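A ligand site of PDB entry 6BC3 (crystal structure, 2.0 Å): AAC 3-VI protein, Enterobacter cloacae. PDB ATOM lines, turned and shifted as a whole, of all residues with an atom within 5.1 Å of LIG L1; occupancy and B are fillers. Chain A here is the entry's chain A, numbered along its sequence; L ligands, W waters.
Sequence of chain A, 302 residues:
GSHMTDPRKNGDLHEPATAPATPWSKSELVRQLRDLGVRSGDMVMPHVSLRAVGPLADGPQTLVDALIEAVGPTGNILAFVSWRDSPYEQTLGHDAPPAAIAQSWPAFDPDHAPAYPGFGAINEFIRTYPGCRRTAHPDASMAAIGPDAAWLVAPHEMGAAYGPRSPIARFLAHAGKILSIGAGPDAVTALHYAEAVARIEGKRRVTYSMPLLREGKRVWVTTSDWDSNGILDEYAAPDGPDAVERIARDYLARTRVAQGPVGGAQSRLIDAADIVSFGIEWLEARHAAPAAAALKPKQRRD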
ATOM      1  N   PRO A  46      27.539   2.497  -8.480  1.00  0.00           N
ATOM      2  CA  PRO A  46      26.984   2.214  -7.143  1.00  0.00           C
ATOM      3  C   PRO A  46      26.865   3.446  -6.256  1.00  0.00           C
ATOM      4  O   PRO A  46      27.695   4.365  -6.279  1.00  0.00           O
ATOM      5  CB  PRO A  46      28.002   1.236  -6.555  1.00  0.00           C
ATOM      6  CG  PRO A  46      29.298   1.651  -7.171  1.00  0.00           C
ATOM      7  CD  PRO A  46      28.970   2.146  -8.564  1.00  0.00           C
ATOM      8  N   HIS A  47      25.786   3.461  -5.476  1.00  0.00           N
ATOM      9  CA  HIS A  47      25.586   4.412  -4.380  1.00  0.00           C
ATOM     10  C   HIS A  47      25.277   3.578  -3.146  1.00  0.00           C
ATOM     11  O   HIS A  47      24.232   2.912  -3.090  1.00  0.00           O
ATOM     12  CB  HIS A  47      24.459   5.399  -4.685  1.00  0.00           C
ATOM     13  CG  HIS A  47      24.691   6.203  -5.926  1.00  0.00           C
ATOM     14  ND1 HIS A  47      25.569   7.267  -5.967  1.00  0.00           N
ATOM     15  CD2 HIS A  47      24.164   6.100  -7.163  1.00  0.00           C
ATOM     16  CE1 HIS A  47      25.565   7.787  -7.183  1.00  0.00           C
ATOM     17  NE2 HIS A  47      24.716   7.097  -7.931  1.00  0.00           N
ATOM     18  N   VAL A  48      26.171   3.600  -2.157  1.00  0.00           N
ATOM     19  CA  VAL A  48      26.193   2.597  -1.107  1.00  0.00           C
ATOM     20  C   VAL A  48      26.092   3.267   0.260  1.00  0.00           C
ATOM     21  O   VAL A  48      26.680   4.332   0.494  1.00  0.00           O
ATOM     22  CB  VAL A  48      27.471   1.732  -1.191  1.00  0.00           C
ATOM     23  CG1 VAL A  48      27.461   0.645  -0.130  1.00  0.00           C
ATOM     24  CG2 VAL A  48      27.607   1.129  -2.585  1.00  0.00           C
ATOM     25  N   SER A  49      25.352   2.628   1.167  1.00  0.00           N
ATOM     26  CA  SER A  49      25.363   2.928   2.592  1.00  0.00           C
ATOM     27  C   SER A  49      25.919   1.695   3.298  1.00  0.00           C
ATOM     28  O   SER A  49      25.226   0.680   3.419  1.00  0.00           O
ATOM     29  CB  SER A  49      23.970   3.279   3.104  1.00  0.00           C
ATOM     30  OG  SER A  49      23.926   3.209   4.525  1.00  0.00           O
ATOM     31  N   LEU A  50      27.174   1.785   3.758  1.00  0.00           N
ATOM     32  CA  LEU A  50      27.816   0.624   4.366  1.00  0.00           C
ATOM     33  C   LEU A  50      27.170   0.247   5.693  1.00  0.00           C
ATOM     34  O   LEU A  50      27.168  -0.931   6.063  1.00  0.00           O
ATOM     35  CB  LEU A  50      29.303   0.888   4.560  1.00  0.00           C
ATOM     36  CG  LEU A  50      30.138   0.845   3.276  1.00  0.00           C
ATOM     37  CD1 LEU A  50      31.582   1.216   3.564  1.00  0.00           C
ATOM     38  CD2 LEU A  50      30.053  -0.532   2.637  1.00  0.00           C
ATOM     39  N   ARG A  51      26.617   1.223   6.431  1.00  0.00           N
ATOM     40  CA  ARG A  51      25.889   0.891   7.648  1.00  0.00           C
ATOM     41  C   ARG A  51      24.636   0.085   7.347  1.00  0.00           C
ATOM     42  O   ARG A  51      24.240  -0.772   8.157  1.00  0.00           O
ATOM     43  CB  ARG A  51      25.538   2.164   8.417  1.00  0.00           C
ATOM     44  CG  ARG A  51      26.739   2.915   8.980  1.00  0.00           C
ATOM     45  CD  ARG A  51      26.294   4.083   9.847  1.00  0.00           C
ATOM     46  NE  ARG A  51      27.420   4.749  10.502  1.00  0.00           N
ATOM     47  CZ  ARG A  51      27.937   5.901  10.105  1.00  0.00           C
ATOM     48  NH1 ARG A  51      27.447   6.530   9.050  1.00  0.00           N
ATOM     49  NH2 ARG A  51      28.964   6.437  10.770  1.00  0.00           N
ATOM     50  N   ALA A  52      24.003   0.333   6.204  1.00  0.00           N
ATOM     51  CA  ALA A  52      22.831  -0.458   5.820  1.00  0.00           C
ATOM     52  C   ALA A  52      23.225  -1.852   5.347  1.00  0.00           C
ATOM     53  O   ALA A  52      22.454  -2.797   5.516  1.00  0.00           O
ATOM     54  CB  ALA A  52      22.041   0.275   4.741  1.00  0.00           C
ATOM     55  N   PRO A  60      34.684  -3.265   4.088  1.00  0.00           N
ATOM     56  CA  PRO A  60      34.129  -2.731   2.827  1.00  0.00           C
ATOM     57  C   PRO A  60      34.771  -3.314   1.570  1.00  0.00           C
ATOM     58  O   PRO A  60      34.144  -3.263   0.503  1.00  0.00           O
ATOM     59  CB  PRO A  60      34.398  -1.228   2.933  1.00  0.00           C
ATOM     60  CG  PRO A  60      34.472  -0.962   4.401  1.00  0.00           C
ATOM     61  CD  PRO A  60      35.101  -2.187   5.006  1.00  0.00           C
ATOM     62  N   PHE A  80      31.078   8.192  -8.389  1.00  0.00           N
ATOM     63  CA  PHE A  80      31.322   9.598  -8.102  1.00  0.00           C
ATOM     64  C   PHE A  80      31.977   9.688  -6.730  1.00  0.00           C
ATOM     65  O   PHE A  80      31.315   9.580  -5.697  1.00  0.00           O
ATOM     66  CB  PHE A  80      30.023  10.400  -8.158  1.00  0.00           C
ATOM     67  CG  PHE A  80      30.170  11.824  -7.705  1.00  0.00           C
ATOM     68  CD1 PHE A  80      29.189  12.414  -6.914  1.00  0.00           C
ATOM     69  CD2 PHE A  80      31.275  12.580  -8.053  1.00  0.00           C
ATOM     70  CE1 PHE A  80      29.306  13.731  -6.495  1.00  0.00           C
ATOM     71  CE2 PHE A  80      31.403  13.889  -7.631  1.00  0.00           C
ATOM     72  CZ  PHE A  80      30.423  14.466  -6.847  1.00  0.00           C
ATOM     73  N   PRO A 117      34.540  11.794   1.887  1.00  0.00           N
ATOM     74  CA  PRO A 117      33.895  10.784   2.747  1.00  0.00           C
ATOM     75  C   PRO A 117      32.385  10.913   2.806  1.00  0.00           C
ATOM     76  O   PRO A 117      31.707   9.903   3.051  1.00  0.00           O
ATOM     77  CB  PRO A 117      34.536  11.038   4.115  1.00  0.00           C
ATOM     78  CG  PRO A 117      35.800  11.793   3.827  1.00  0.00           C
ATOM     79  CD  PRO A 117      35.495  12.637   2.629  1.00  0.00           C
ATOM     80  N   GLY A 118      31.839  12.106   2.579  1.00  0.00           N
ATOM     81  CA  GLY A 118      30.401  12.296   2.686  1.00  0.00           C
ATOM     82  C   GLY A 118      29.595  11.567   1.640  1.00  0.00           C
ATOM     83  O   GLY A 118      28.393  11.355   1.841  1.00  0.00           O
ATOM     84  N   PHE A 119      30.205  11.170   0.536  1.00  0.00           N
ATOM     85  CA  PHE A 119      29.518  10.465  -0.531  1.00  0.00           C
ATOM     86  C   PHE A 119      29.624   8.956  -0.406  1.00  0.00           C
ATOM     87  O   PHE A 119      29.265   8.231  -1.346  1.00  0.00           O
ATOM     88  CB  PHE A 119      30.037  10.924  -1.899  1.00  0.00           C
ATOM     89  CG  PHE A 119      29.867  12.402  -2.154  1.00  0.00           C
ATOM     90  CD1 PHE A 119      28.840  13.104  -1.543  1.00  0.00           C
ATOM     91  CD2 PHE A 119      30.733  13.072  -2.991  1.00  0.00           C
ATOM     92  CE1 PHE A 119      28.672  14.453  -1.773  1.00  0.00           C
ATOM     93  CE2 PHE A 119      30.574  14.429  -3.232  1.00  0.00           C
ATOM     94  CZ  PHE A 119      29.548  15.122  -2.618  1.00  0.00           C
ATOM     95  N   GLY A 120      30.120   8.453   0.728  1.00  0.00           N
ATOM     96  CA  GLY A 120      30.197   7.014   0.925  1.00  0.00           C
ATOM     97  C   GLY A 120      31.627   6.573   1.188  1.00  0.00           C
ATOM     98  O   GLY A 120      32.538   6.848   0.413  1.00  0.00           O
ATOM     99  N   ALA A 121      31.811   5.862   2.301  1.00  0.00           N
ATOM    100  CA  ALA A 121      33.118   5.320   2.648  1.00  0.00           C
ATOM    101  C   ALA A 121      33.585   4.265   1.658  1.00  0.00           C
ATOM    102  O   ALA A 121      34.780   3.966   1.609  1.00  0.00           O
ATOM    103  CB  ALA A 121      33.101   4.737   4.057  1.00  0.00           C
ATOM    104  N   ILE A 122      32.656   3.686   0.885  1.00  0.00           N
ATOM    105  CA  ILE A 122      33.020   2.666  -0.099  1.00  0.00           C
ATOM    106  C   ILE A 122      33.920   3.259  -1.183  1.00  0.00           C
ATOM    107  O   ILE A 122      34.728   2.539  -1.790  1.00  0.00           O
ATOM    108  CB  ILE A 122      31.749   2.037  -0.690  1.00  0.00           C
ATOM    109  CG1 ILE A 122      32.087   0.825  -1.571  1.00  0.00           C
ATOM    110  CG2 ILE A 122      30.964   3.056  -1.495  1.00  0.00           C
ATOM    111  CD1 ILE A 122      32.126  -0.479  -0.810  1.00  0.00           C
ATOM    112  N   ASN A 123      33.797   4.563  -1.439  1.00  0.00           N
ATOM    113  CA  ASN A 123      34.459   5.146  -2.594  1.00  0.00           C
ATOM    114  C   ASN A 123      35.977   5.202  -2.444  1.00  0.00           C
ATOM    115  O   ASN A 123      36.695   5.138  -3.437  1.00  0.00           O
ATOM    116  CB  ASN A 123      33.896   6.543  -2.869  1.00  0.00           C
ATOM    117  CG  ASN A 123      32.500   6.497  -3.462  1.00  0.00           C
ATOM    118  OD1 ASN A 123      32.156   5.557  -4.175  1.00  0.00           O
ATOM    119  ND2 ASN A 123      31.704   7.522  -3.178  1.00  0.00           N
ATOM    120  N   PHE A 125      37.642   2.834  -1.028  1.00  0.00           N
ATOM    121  CA  PHE A 125      38.039   1.483  -1.388  1.00  0.00           C
ATOM    122  C   PHE A 125      37.971   1.270  -2.892  1.00  0.00           C
ATOM    123  O   PHE A 125      38.807   0.562  -3.470  1.00  0.00           O
ATOM    124  CB  PHE A 125      37.168   0.461  -0.652  1.00  0.00           C
ATOM    125  CG  PHE A 125      37.468   0.350   0.819  1.00  0.00           C
ATOM    126  CD1 PHE A 125      38.366  -0.598   1.289  1.00  0.00           C
ATOM    127  CD2 PHE A 125      36.851   1.192   1.726  1.00  0.00           C
ATOM    128  CE1 PHE A 125      38.639  -0.705   2.633  1.00  0.00           C
ATOM    129  CE2 PHE A 125      37.134   1.088   3.080  1.00  0.00           C
ATOM    130  CZ  PHE A 125      38.022   0.146   3.537  1.00  0.00           C
ATOM    131  N   GLY A 182      21.154   0.579  -0.361  1.00  0.00           N
ATOM    132  CA  GLY A 182      20.797   1.234   0.882  1.00  0.00           C
ATOM    133  C   GLY A 182      20.848   2.754   0.856  1.00  0.00           C
ATOM    134  O   GLY A 182      20.670   3.378   1.899  1.00  0.00           O
ATOM    135  N   ALA A 183      21.077   3.351  -0.307  1.00  0.00           N
ATOM    136  CA  ALA A 183      21.158   4.792  -0.434  1.00  0.00           C
ATOM    137  C   ALA A 183      19.788   5.375  -0.765  1.00  0.00           C
ATOM    138  O   ALA A 183      18.962   4.727  -1.408  1.00  0.00           O
ATOM    139  CB  ALA A 183      22.176   5.201  -1.501  1.00  0.00           C
ATOM    140  N   GLY A 184      19.560   6.608  -0.320  1.00  0.00           N
ATOM    141  CA  GLY A 184      18.309   7.288  -0.567  1.00  0.00           C
ATOM    142  C   GLY A 184      18.194   7.772  -1.987  1.00  0.00           C
ATOM    143  O   GLY A 184      19.153   7.753  -2.782  1.00  0.00           O
ATOM    144  N   ASP A 186      18.076  10.689  -3.067  1.00  0.00           N
ATOM    145  CA  ASP A 186      18.889  11.862  -3.329  1.00  0.00           C
ATOM    146  C   ASP A 186      20.264  11.515  -3.896  1.00  0.00           C
ATOM    147  O   ASP A 186      20.949  12.410  -4.399  1.00  0.00           O
ATOM    148  CB  ASP A 186      19.078  12.678  -2.050  1.00  0.00           C
ATOM    149  CG  ASP A 186      19.920  11.949  -1.010  1.00  0.00           C
ATOM    150  OD1 ASP A 186      19.471  10.895  -0.512  1.00  0.00           O
ATOM    151  OD2 ASP A 186      21.043  12.419  -0.716  1.00  0.00           O
ATOM    152  N   ALA A 187      20.670  10.253  -3.833  1.00  0.00           N
ATOM    153  CA  ALA A 187      22.023   9.863  -4.213  1.00  0.00           C
ATOM    154  C   ALA A 187      22.186   9.650  -5.714  1.00  0.00           C
ATOM    155  O   ALA A 187      23.324   9.440  -6.165  1.00  0.00           O
ATOM    156  CB  ALA A 187      22.431   8.586  -3.470  1.00  0.00           C
ATOM    157  N   VAL A 188      21.109   9.702  -6.494  1.00  0.00           N
ATOM    158  CA  VAL A 188      21.194   9.447  -7.936  1.00  0.00           C
ATOM    159  C   VAL A 188      21.952  10.583  -8.607  1.00  0.00           C
ATOM    160  O   VAL A 188      21.349  11.515  -9.149  1.00  0.00           O
ATOM    161  CB  VAL A 188      19.802   9.259  -8.552  1.00  0.00           C
ATOM    162  CG1 VAL A 188      19.919   8.768  -9.989  1.00  0.00           C
ATOM    163  CG2 VAL A 188      18.984   8.282  -7.711  1.00  0.00           C
ATOM    164  N   THR A 189      23.285  10.501  -8.594  1.00  0.00           N
ATOM    165  CA  THR A 189      24.117  11.561  -9.146  1.00  0.00           C
ATOM    166  C   THR A 189      23.891  11.756 -10.637  1.00  0.00           C
ATOM    167  O   THR A 189      23.993  12.873 -11.140  1.00  0.00           O
ATOM    168  CB  THR A 189      25.593  11.264  -8.869  1.00  0.00           C
ATOM    169  OG1 THR A 189      25.795  11.141  -7.451  1.00  0.00           O
ATOM    170  CG2 THR A 189      26.490  12.381  -9.391  1.00  0.00           C
HETATM  171  N1  LIG L   1      37.423   0.775   6.967  1.00  0.00           N
HETATM  172  C1  LIG L   1      36.380   0.223   7.647  1.00  0.00           C
HETATM  173  N2  LIG L   1      35.251   0.941   7.905  1.00  0.00           N
HETATM  174  C2  LIG L   1      35.154   2.237   7.465  1.00  0.00           C
HETATM  175  C3  LIG L   1      36.177   2.781   6.798  1.00  0.00           C
HETATM  176  C4  LIG L   1      37.329   2.026   6.551  1.00  0.00           C
HETATM  177  N3  LIG L   1      38.533   2.362   5.868  1.00  0.00           N
HETATM  178  N4  LIG L   1      35.858   4.050   6.478  1.00  0.00           N
HETATM  179  C5  LIG L   1      34.628   4.271   6.963  1.00  0.00           C
HETATM  180  N5  LIG L   1      34.191   3.163   7.560  1.00  0.00           N
HETATM  181  C6  LIG L   1      32.936   2.951   8.216  1.00  0.00           C
HETATM  182  C7  LIG L   1      32.575   4.073   8.788  1.00  0.00           C
HETATM  183  O1  LIG L   1      33.393   4.319   9.928  1.00  0.00           O
HETATM  184  C8  LIG L   1      31.129   3.730   9.148  1.00  0.00           C
HETATM  185  O2  LIG L   1      31.115   2.742  10.046  1.00  0.00           O
HETATM  186  P1  LIG L   1      30.821   3.135  11.667  1.00  0.00           P
HETATM  187  O3  LIG L   1      29.719   4.160  11.748  1.00  0.00           O
HETATM  188  O4  LIG L   1      32.107   3.697  12.309  1.00  0.00           O
HETATM  189  O5  LIG L   1      30.393   1.888  12.397  1.00  0.00           O
HETATM  190  C9  LIG L   1      30.637   3.182   7.767  1.00  0.00           C
HETATM  191  O6  LIG L   1      31.671   2.602   7.215  1.00  0.00           O
HETATM  192  C10 LIG L   1      30.211   4.362   6.905  1.00  0.00           C
HETATM  193  O7  LIG L   1      29.399   3.912   5.853  1.00  0.00           O
HETATM  194  P2  LIG L   1      28.925   5.033   4.725  1.00  0.00           P
HETATM  195  O8  LIG L   1      30.130   5.834   4.286  1.00  0.00           O
HETATM  196  O9  LIG L   1      28.395   4.302   3.517  1.00  0.00           O
HETATM  197  O10 LIG L   1      27.779   6.039   5.380  1.00  0.00           O
HETATM  198  P3  LIG L   1      26.213   5.460   5.789  1.00  0.00           P
HETATM  199  O11 LIG L   1      25.817   5.939   7.193  1.00  0.00           O
HETATM  200  O12 LIG L   1      26.173   3.940   5.774  1.00  0.00           O
HETATM  201  O13 LIG L   1      25.121   6.092   4.701  1.00  0.00           O
HETATM  202  C11 LIG L   1      25.464   7.700   2.951  1.00  0.00           C
HETATM  203  C12 LIG L   1      25.231   7.478   4.445  1.00  0.00           C
HETATM  204  C13 LIG L   1      26.855   7.329   2.589  1.00  0.00           C
HETATM  205  C14 LIG L   1      25.278   9.164   2.615  1.00  0.00           C
HETATM  206  C15 LIG L   1      24.430   6.848   2.165  1.00  0.00           C
HETATM  207  O14 LIG L   1      23.202   7.025   2.714  1.00  0.00           O
HETATM  208  C16 LIG L   1      24.401   7.299   0.676  1.00  0.00           C
HETATM  209  O15 LIG L   1      23.520   8.033   0.288  1.00  0.00           O
HETATM  210  N6  LIG L   1      25.496   6.828  -0.246  1.00  0.00           N
HETATM  211  C17 LIG L   1      25.493   7.305  -1.689  1.00  0.00           C
HETATM  212  C18 LIG L   1      25.989   8.756  -1.609  1.00  0.00           C
HETATM  213  C19 LIG L   1      26.461   9.294  -2.981  1.00  0.00           C
HETATM  214  O16 LIG L   1      26.795   8.565  -3.851  1.00  0.00           O
HETATM  215  N7  LIG L   1      26.519  10.685  -3.168  1.00  0.00           N
HETATM  216  C20 LIG L   1      26.958  11.218  -4.436  1.00  0.00           C
HETATM  217  C21 LIG L   1      26.392  12.670  -4.477  1.00  0.00           C
HETATM  218  S1  LIG L   1      24.561  12.523  -4.598  1.00  0.00           S
HETATM  219  C1  LG2 L   2      23.981  16.242  -1.643  1.00  0.00           C
HETATM  220  C2  LG2 L   2      27.520  17.259  -5.362  1.00  0.00           C
HETATM  221  C3  LG2 L   2      28.948  19.688  -3.768  1.00  0.00           C
HETATM  222  C4  LG2 L   2      23.519  15.181  -1.019  1.00  0.00           C
HETATM  223  C5  LG2 L   2      26.134  16.911  -5.995  1.00  0.00           C
HETATM  224  C6  LG2 L   2      30.485  19.712  -3.847  1.00  0.00           C
HETATM  225  C7  LG2 L   2      22.505  15.538   0.250  1.00  0.00           C
HETATM  226  C8  LG2 L   2      25.319  15.972  -5.019  1.00  0.00           C
HETATM  227  C9  LG2 L   2      31.051  19.171  -2.574  1.00  0.00           C
HETATM  228  C10 LG2 L   2      21.581  16.498  -0.026  1.00  0.00           C
HETATM  229  C11 LG2 L   2      25.149  16.735  -3.672  1.00  0.00           C
HETATM  230  C12 LG2 L   2      30.583  19.956  -1.394  1.00  0.00           C
HETATM  231  C13 LG2 L   2      21.956  17.563  -1.124  1.00  0.00           C
HETATM  232  C14 LG2 L   2      26.434  17.452  -3.146  1.00  0.00           C
HETATM  233  C15 LG2 L   2      29.042  20.090  -1.349  1.00  0.00           C
HETATM  234  C16 LG2 L   2      21.404  18.943  -1.060  1.00  0.00           C
HETATM  235  C17 LG2 L   2      27.306  18.119  -4.179  1.00  0.00           C
HETATM  236  C18 LG2 L   2      31.031  19.263  -0.075  1.00  0.00           C
HETATM  237  C19 LG2 L   2      33.130  17.882  -2.590  1.00  0.00           C
HETATM  238  N1  LG2 L   2      28.404  17.897  -6.355  1.00  0.00           N
HETATM  239  N2  LG2 L   2      22.769  14.252  -1.975  1.00  0.00           N
HETATM  240  N3  LG2 L   2      24.063  15.704  -5.553  1.00  0.00           N
HETATM  241  N4  LG2 L   2      32.566  19.229  -2.674  1.00  0.00           N
HETATM  242  N5  LG2 L   2      21.591  19.706  -2.323  1.00  0.00           N
HETATM  243  O1  LG2 L   2      24.763  15.748  -2.773  1.00  0.00           O
HETATM  244  O2  LG2 L   2      30.893  18.895  -4.938  1.00  0.00           O
HETATM  245  O3  LG2 L   2      31.157  21.262  -1.446  1.00  0.00           O
HETATM  246  O4  LG2 L   2      22.823  17.204  -2.172  1.00  0.00           O
HETATM  247  O5  LG2 L   2      26.075  18.425  -2.180  1.00  0.00           O
HETATM  248  O6  LG2 L   2      28.457  20.518  -2.644  1.00  0.00           O
HETATM  249  O7  LG2 L   2      28.609  18.396  -3.551  1.00  0.00           O
HETATM  250  O   HOH W   1      20.842   8.993   0.904  1.00  0.00           O
HETATM  251  O   HOH W   2      29.204   8.031  -4.870  1.00  0.00           O
HETATM  252  O   HOH W   3      36.659   4.994   3.535  1.00  0.00           O
HETATM  253  O   HOH W   4      23.213  10.919   0.298  1.00  0.00           O
HETATM  254  O   HOH W   5      28.259   5.494  -2.280  1.00  0.00           O
HETATM  255  O   HOH W   6      29.552   3.862   1.364  1.00  0.00           O
HETATM  256  O   HOH W   7      27.685   3.990  13.150  1.00  0.00           O
HETATM  257  O   HOH W   8      25.093  12.103  -1.125  1.00  0.00           O
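Water W7 lies within hydrogen-bond range of an oxygen (O3) of LIG L1 and the guanidinium group (NE) of Arg 51. Water W2 lies within hydrogen-bond range of O16 of LIG L1 (2.7 Å), O of Phe 80 (2.7 Å) and ND2 of Asn 123 (3.1 Å). Water W8 bridges a nitrogen (N7) of LIG L1 (2.9 Å) and a nitrogen (N2) of LG2 L2 (3.3 Å). Water W1 lies within hydrogen-bond range of OD1 of Asp 186 (2.7 Å), O15 of LIG L1 (2.9 Å) and N of Gly 184 (3.0 Å). Water W3 lies within hydrogen-bond range of the backbone carbonyl oxygen (O) of Ala 121 and a nitrogen (N4) of LIG L1. Water W5 bridges N of Val 48 (2.8 Å) and O of Phe 119 (3.1 Å).
OG1 of Thr 189 sits close to S1 of LIG L1, at 3.4 Å. A ring nitrogen (ND1) of His 47 sits at hydrogen-bond distance from an oxygen (O16) of LIG L1 (2.8 Å). The backbone carbonyl oxygen (O) of Ala 187 lies close to a sulfur (S1) of LIG L1, 3.7 Å away. An oxygen (O9) of LIG L1 lies within hydrogen-bond range of the backbone NH of Leu 50 (2.8 Å). An oxygen (O12) of LIG L1 lies within hydrogen-bond range of the backbone NH (N) of Arg 51, 2.8 Å away. An oxygen (O12) of LIG L1 lies within hydrogen-bond range of the side-chain hydroxyl (OG) of Ser 49 (2.7 Å). O of Asp 186 sits close to S1 of LIG L1. N of Ala 121 sits at hydrogen-bond distance from O8 of LIG L1 (2.6 Å). NH1 of Arg 51 is in salt-bridge range of O11 of LIG L1 (2.5 Å). The backbone carbonyl oxygen of Val 48 sits at hydrogen-bond distance from a nitrogen (N6) of LIG L1 (2.9 Å). OD2 of Asp 186 lies within salt-bridge range of N2 of LG2 L2 (2.8 Å).
S1 of LIG L1 lies close to N3 of LG2 L2 (3.4 Å).
Pro 60 touches LIG L1 (CD to C1, 3.8 Å). Phe 80 touches LIG L1 (CD1 to C20, 3.5 Å). Gly 118 touches LIG L1 (O to C14, 3.9 Å). Phe 119 touches LIG L1 (O to C18, 3.3 Å). Gly 120 touches LIG L1 (C to O8, 3.5 Å). Phe 125 touches LIG L1. Ala 183 touches LIG L1 (CB to O15, 3.6 Å). Hydrophobic or aromatic side chains that line LIG L1: His 47, Leu 50, Pro 60, Phe 80, Phe 119, Ala 121, Phe 125, Ala 183 and Ala 187. Of the 24 residues printed, 16 come within 4 Å of LIG L1. The nearest printed residue that does not touch LIG L1 is Ala 52 (4.2 Å).
The backbone carbonyl oxygen (O) of Phe 119 sits at hydrogen-bond distance from the side-chain amide nitrogen (ND2) of Asn 123 (3.1 Å). The backbone carbonyl oxygen of Phe 80 lies within hydrogen-bond range of the side-chain amide nitrogen of Asn 123, at 3.3 Å. A ring nitrogen (ND1) of His 47 sits close to the backbone carbonyl oxygen of Ala 187, at 3.1 Å. OG1 of Thr 189 is in hydrogen-bond range of O of Ala 187 (3.3 Å). OG of Ser 49 is in hydrogen-bond range of N of Ala 52.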
